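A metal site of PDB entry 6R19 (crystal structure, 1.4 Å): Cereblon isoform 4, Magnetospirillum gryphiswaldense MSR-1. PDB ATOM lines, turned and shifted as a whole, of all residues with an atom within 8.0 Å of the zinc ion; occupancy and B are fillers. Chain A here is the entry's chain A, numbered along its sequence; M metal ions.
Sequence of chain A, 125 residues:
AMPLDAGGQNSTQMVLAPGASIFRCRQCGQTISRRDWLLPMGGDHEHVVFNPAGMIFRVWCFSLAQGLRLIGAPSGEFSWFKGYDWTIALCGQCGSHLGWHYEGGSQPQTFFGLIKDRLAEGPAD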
ATOM      1  N   ARG A  24      25.578 -20.132  19.133  1.00  0.00           N
ATOM      2  CA  ARG A  24      24.133 -20.154  19.180  1.00  0.00           C
ATOM      3  C   ARG A  24      23.559 -18.885  18.587  1.00  0.00           C
ATOM      4  O   ARG A  24      24.224 -17.877  18.520  1.00  0.00           O
ATOM      5  CB  ARG A  24      23.709 -20.250  20.668  1.00  0.00           C
ATOM      6  CG  ARG A  24      24.060 -21.539  21.322  1.00  0.00           C
ATOM      7  CD  ARG A  24      23.561 -21.702  22.765  1.00  0.00           C
ATOM      8  NE  ARG A  24      23.880 -23.006  23.288  1.00  0.00           N
ATOM      9  CZ  ARG A  24      23.322 -24.119  22.895  1.00  0.00           C
ATOM     10  NH1 ARG A  24      22.169 -24.110  22.213  1.00  0.00           N
ATOM     11  NH2 ARG A  24      23.790 -25.254  23.299  1.00  0.00           N
ATOM     12  N   CYS A  25      22.290 -18.898  18.188  1.00  0.00           N
ATOM     13  CA  CYS A  25      21.610 -17.699  17.767  1.00  0.00           C
ATOM     14  C   CYS A  25      21.580 -16.708  18.915  1.00  0.00           C
ATOM     15  O   CYS A  25      21.201 -17.057  20.048  1.00  0.00           O
ATOM     16  CB  CYS A  25      20.216 -18.047  17.302  1.00  0.00           C
ATOM     17  SG  CYS A  25      19.213 -16.565  16.925  1.00  0.00           S
ATOM     18  N   ARG A  26      22.051 -15.488  18.672  1.00  0.00           N
ATOM     19  CA  ARG A  26      22.064 -14.450  19.712  1.00  0.00           C
ATOM     20  C   ARG A  26      20.710 -14.073  20.238  1.00  0.00           C
ATOM     21  O   ARG A  26      20.586 -13.627  21.392  1.00  0.00           O
ATOM     22  CB  ARG A  26      22.773 -13.230  19.168  1.00  0.00           C
ATOM     23  CG  ARG A  26      22.821 -12.065  20.062  1.00  0.00           C
ATOM     24  CD  ARG A  26      23.589 -10.941  19.403  1.00  0.00           C
ATOM     25  NE  ARG A  26      23.503  -9.762  20.233  1.00  0.00           N
ATOM     26  CZ  ARG A  26      24.085  -8.597  19.958  1.00  0.00           C
ATOM     27  NH1 ARG A  26      24.844  -8.467  18.869  1.00  0.00           N
ATOM     28  NH2 ARG A  26      23.890  -7.573  20.752  1.00  0.00           N
ATOM     29  N   GLN A  27      19.701 -14.239  19.387  1.00  0.00           N
ATOM     30  CA  GLN A  27      18.334 -13.807  19.782  1.00  0.00           C
ATOM     31  C   GLN A  27      17.617 -14.843  20.563  1.00  0.00           C
ATOM     32  O   GLN A  27      16.770 -14.460  21.374  1.00  0.00           O
ATOM     33  CB  GLN A  27      17.562 -13.371  18.573  1.00  0.00           C
ATOM     34  CG  GLN A  27      18.192 -12.250  17.866  1.00  0.00           C
ATOM     35  CD  GLN A  27      18.391 -11.005  18.718  1.00  0.00           C
ATOM     36  OE1 GLN A  27      17.546 -10.667  19.490  1.00  0.00           O
ATOM     37  NE2 GLN A  27      19.564 -10.360  18.606  1.00  0.00           N
ATOM     38  N   CYS A  28      17.879 -16.134  20.430  1.00  0.00           N
ATOM     39  CA  CYS A  28      17.056 -17.160  21.051  1.00  0.00           C
ATOM     40  C   CYS A  28      17.803 -18.316  21.626  1.00  0.00           C
ATOM     41  O   CYS A  28      17.223 -19.132  22.381  1.00  0.00           O
ATOM     42  CB  CYS A  28      15.986 -17.633  20.091  1.00  0.00           C
ATOM     43  SG  CYS A  28      16.659 -18.742  18.803  1.00  0.00           S
ATOM     44  N   GLY A  29      19.076 -18.515  21.302  1.00  0.00           N
ATOM     45  CA  GLY A  29      19.771 -19.653  21.814  1.00  0.00           C
ATOM     46  C   GLY A  29      19.851 -20.932  21.039  1.00  0.00           C
ATOM     47  O   GLY A  29      20.564 -21.855  21.423  1.00  0.00           O
ATOM     48  N   GLN A  30      19.152 -20.963  19.872  1.00  0.00           N
ATOM     49  CA  GLN A  30      19.243 -22.133  19.003  1.00  0.00           C
ATOM     50  C   GLN A  30      20.708 -22.518  18.738  1.00  0.00           C
ATOM     51  O   GLN A  30      21.465 -21.669  18.399  1.00  0.00           O
ATOM     52  CB  GLN A  30      18.594 -21.762  17.677  1.00  0.00           C
ATOM     53  CG  GLN A  30      18.667 -22.813  16.575  1.00  0.00           C
ATOM     54  CD  GLN A  30      17.628 -23.856  16.746  1.00  0.00           C
ATOM     55  OE1 GLN A  30      17.435 -24.420  17.862  1.00  0.00           O
ATOM     56  NE2 GLN A  30      16.977 -24.184  15.634  1.00  0.00           N
ATOM     57  N   THR A  31      21.043 -23.810  18.822  1.00  0.00           N
ATOM     58  CA  THR A  31      22.403 -24.247  18.437  1.00  0.00           C
ATOM     59  C   THR A  31      22.584 -24.087  16.935  1.00  0.00           C
ATOM     60  O   THR A  31      21.733 -24.551  16.219  1.00  0.00           O
ATOM     61  CB  THR A  31      22.562 -25.733  18.771  1.00  0.00           C
ATOM     62  OG1 THR A  31      22.010 -26.013  20.076  1.00  0.00           O
ATOM     63  CG2 THR A  31      23.957 -26.070  18.727  1.00  0.00           C
ATOM     64  N   ILE A  32      23.666 -23.436  16.506  1.00  0.00           N
ATOM     65  CA  ILE A  32      23.899 -23.135  15.075  1.00  0.00           C
ATOM     66  C   ILE A  32      25.211 -23.765  14.569  1.00  0.00           C
ATOM     67  O   ILE A  32      25.215 -24.379  13.521  1.00  0.00           O
ATOM     68  CB  ILE A  32      23.898 -21.642  14.797  1.00  0.00           C
ATOM     69  CG1 ILE A  32      22.608 -20.963  15.207  1.00  0.00           C
ATOM     70  CG2 ILE A  32      24.180 -21.401  13.319  1.00  0.00           C
ATOM     71  CD1 ILE A  32      21.381 -21.430  14.540  1.00  0.00           C
ATOM     72  N   GLY A  67      20.344 -26.016  12.769  1.00  0.00           N
ATOM     73  CA  GLY A  67      19.384 -25.158  13.390  1.00  0.00           C
ATOM     74  C   GLY A  67      18.911 -24.004  12.582  1.00  0.00           C
ATOM     75  O   GLY A  67      18.245 -23.089  13.120  1.00  0.00           O
ATOM     76  N   LEU A  68      19.227 -23.965  11.299  1.00  0.00           N
ATOM     77  CA  LEU A  68      18.832 -22.897  10.407  1.00  0.00           C
ATOM     78  C   LEU A  68      17.657 -23.351   9.604  1.00  0.00           C
ATOM     79  O   LEU A  68      17.276 -24.526   9.621  1.00  0.00           O
ATOM     80  CB  LEU A  68      19.990 -22.551   9.456  1.00  0.00           C
ATOM     81  CG  LEU A  68      21.214 -22.007  10.158  1.00  0.00           C
ATOM     82  CD1 LEU A  68      22.418 -22.146   9.240  1.00  0.00           C
ATOM     83  CD2 LEU A  68      21.068 -20.570  10.641  1.00  0.00           C
ATOM     84  N   LEU A  90      17.967 -18.383   7.844  1.00  0.00           N
ATOM     85  CA  LEU A  90      17.365 -17.850   9.074  1.00  0.00           C
ATOM     86  C   LEU A  90      17.609 -18.811  10.195  1.00  0.00           C
ATOM     87  O   LEU A  90      17.745 -20.019   9.988  1.00  0.00           O
ATOM     88  CB  LEU A  90      15.871 -17.666   8.877  1.00  0.00           C
ATOM     89  CG  LEU A  90      15.419 -16.825   7.654  1.00  0.00           C
ATOM     90  CD1 LEU A  90      13.908 -16.715   7.681  1.00  0.00           C
ATOM     91  CD2 LEU A  90      16.117 -15.458   7.668  1.00  0.00           C
ATOM     92  N   CYS A  91      17.634 -18.297  11.407  1.00  0.00           N
ATOM     93  CA  CYS A  91      17.478 -19.153  12.589  1.00  0.00           C
ATOM     94  C   CYS A  91      16.209 -19.931  12.423  1.00  0.00           C
ATOM     95  O   CYS A  91      15.117 -19.369  12.209  1.00  0.00           O
ATOM     96  CB  CYS A  91      17.501 -18.339  13.843  1.00  0.00           C
ATOM     97  SG  CYS A  91      17.246 -19.363  15.323  1.00  0.00           S
ATOM     98  N   GLY A  92      16.300 -21.275  12.534  1.00  0.00           N
ATOM     99  CA  GLY A  92      15.127 -22.083  12.403  1.00  0.00           C
ATOM    100  C   GLY A  92      14.167 -21.984  13.523  1.00  0.00           C
ATOM    101  O   GLY A  92      13.036 -22.448  13.347  1.00  0.00           O
ATOM    102  N   GLN A  93      14.576 -21.461  14.664  1.00  0.00           N
ATOM    103  CA  GLN A  93      13.745 -21.330  15.828  1.00  0.00           C
ATOM    104  C   GLN A  93      13.041 -19.972  15.784  1.00  0.00           C
ATOM    105  O   GLN A  93      11.849 -19.876  15.754  1.00  0.00           O
ATOM    106  CB  GLN A  93      14.591 -21.543  17.058  1.00  0.00           C
ATOM    107  CG  GLN A  93      13.876 -21.424  18.360  1.00  0.00           C
ATOM    108  CD  GLN A  93      14.602 -22.148  19.492  1.00  0.00           C
ATOM    109  OE1 GLN A  93      14.316 -23.320  19.745  1.00  0.00           O
ATOM    110  NE2 GLN A  93      15.561 -21.486  20.099  1.00  0.00           N
ATOM    111  N   CYS A  94      13.823 -18.898  15.738  1.00  0.00           N
ATOM    112  CA  CYS A  94      13.202 -17.535  15.901  1.00  0.00           C
ATOM    113  C   CYS A  94      13.098 -16.707  14.608  1.00  0.00           C
ATOM    114  O   CYS A  94      12.449 -15.660  14.648  1.00  0.00           O
ATOM    115  CB  CYS A  94      13.970 -16.749  16.898  1.00  0.00           C
ATOM    116  SG  CYS A  94      15.538 -15.992  16.344  1.00  0.00           S
ATOM    117  N   GLY A  95      13.734 -17.162  13.511  1.00  0.00           N
ATOM    118  CA  GLY A  95      13.609 -16.424  12.256  1.00  0.00           C
ATOM    119  C   GLY A  95      14.612 -15.341  12.045  1.00  0.00           C
ATOM    120  O   GLY A  95      14.619 -14.718  10.980  1.00  0.00           O
ATOM    121  N   SER A  96      15.492 -15.094  12.975  1.00  0.00           N
ATOM    122  CA  SER A  96      16.577 -14.089  12.853  1.00  0.00           C
ATOM    123  C   SER A  96      17.419 -14.424  11.602  1.00  0.00           C
ATOM    124  O   SER A  96      17.758 -15.582  11.362  1.00  0.00           O
ATOM    125  CB  SER A  96      17.479 -14.120  14.069  1.00  0.00           C
ATOM    126  OG  SER A  96      18.593 -13.203  13.949  1.00  0.00           O
ATOM    127  N   HIS A  97      17.787 -13.385  10.838  1.00  0.00           N
ATOM    128  CA  HIS A  97      18.629 -13.643   9.682  1.00  0.00           C
ATOM    129  C   HIS A  97      20.070 -13.826  10.099  1.00  0.00           C
ATOM    130  O   HIS A  97      20.696 -12.855  10.510  1.00  0.00           O
ATOM    131  CB  HIS A  97      18.463 -12.524   8.641  1.00  0.00           C
ATOM    132  CG  HIS A  97      19.370 -12.690   7.505  1.00  0.00           C
ATOM    133  ND1 HIS A  97      19.858 -11.591   6.789  1.00  0.00           N
ATOM    134  CD2 HIS A  97      19.868 -13.802   6.929  1.00  0.00           C
ATOM    135  CE1 HIS A  97      20.630 -12.086   5.834  1.00  0.00           C
ATOM    136  NE2 HIS A  97      20.636 -13.409   5.876  1.00  0.00           N
ATOM    137  N   LEU A  98      20.585 -15.038  10.076  1.00  0.00           N
ATOM    138  CA  LEU A  98      21.899 -15.345  10.535  1.00  0.00           C
ATOM    139  C   LEU A  98      22.946 -15.379   9.489  1.00  0.00           C
ATOM    140  O   LEU A  98      24.137 -15.300   9.806  1.00  0.00           O
ATOM    141  CB  LEU A  98      21.910 -16.666  11.332  1.00  0.00           C
ATOM    142  CG  LEU A  98      21.046 -16.643  12.602  1.00  0.00           C
ATOM    143  CD1 LEU A  98      21.251 -17.951  13.381  1.00  0.00           C
ATOM    144  CD2 LEU A  98      21.324 -15.438  13.510  1.00  0.00           C
ATOM    145  N   ARG A 118      25.652 -11.790  15.022  1.00  0.00           N
ATOM    146  CA  ARG A 118      24.334 -12.332  15.240  1.00  0.00           C
ATOM    147  C   ARG A 118      24.371 -13.649  15.953  1.00  0.00           C
ATOM    148  O   ARG A 118      23.286 -14.325  16.143  1.00  0.00           O
ATOM    149  CB  ARG A 118      23.561 -12.382  13.945  1.00  0.00           C
ATOM    150  CG  ARG A 118      23.417 -10.978  13.361  1.00  0.00           C
ATOM    151  CD  ARG A 118      22.494 -10.906  12.175  1.00  0.00           C
ATOM    152  NE  ARG A 118      22.549  -9.600  11.552  1.00  0.00           N
ATOM    153  CZ  ARG A 118      21.783  -9.215  10.537  1.00  0.00           C
ATOM    154  NH1 ARG A 118      20.930 -10.029  10.004  1.00  0.00           N
ATOM    155  NH2 ARG A 118      21.909  -7.981  10.006  1.00  0.00           N
HETATM  156 ZN    ZN M   1      17.170 -17.566  16.894  1.00  0.00          ZN
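The backbone NH of Cys 25 is in hydrogen-bond range of the backbone carbonyl oxygen of Gln 30, at 2.9 Å.
N of Cys 91 is in hydrogen-bond range of O of Ser 96 (2.7 Å).
The side-chain sulfur of Cys 91 sits close to the backbone NH of Gln 93 (3.5 Å).
The side-chain sulfur (SG) of Cys 94 lies close to the backbone NH (N) of Ser 96, 3.5 Å away.
The side-chain sulfur (SG) of Cys 25 lies close to the backbone NH (N) of Gln 27.
The backbone NH (N) of Gln 30 sits close to the side-chain sulfur (SG) of Cys 28 (3.5 Å).
SG of Cys 28 lies close to NE2 of Gln 93 (3.2 Å).
Within 4 Å of the zinc ion: Cys 25, Cys 28, Cys 91 and Cys 94.
The nearest printed residue that does not touch the zinc ion is Ser 96 (4.5 Å).
The zinc ion is bound by SG of Cys 25, at 2.3 Å.
SG of Cys 28 binds the zinc ion (2.3 Å).
The zinc ion is bound by the side-chain sulfur (SG) of Cys 94, at 2.3 Å.
SG of Cys 91 is bound to the zinc ion (2.4 Å).
The zinc ion has four donor atoms within binding distance.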
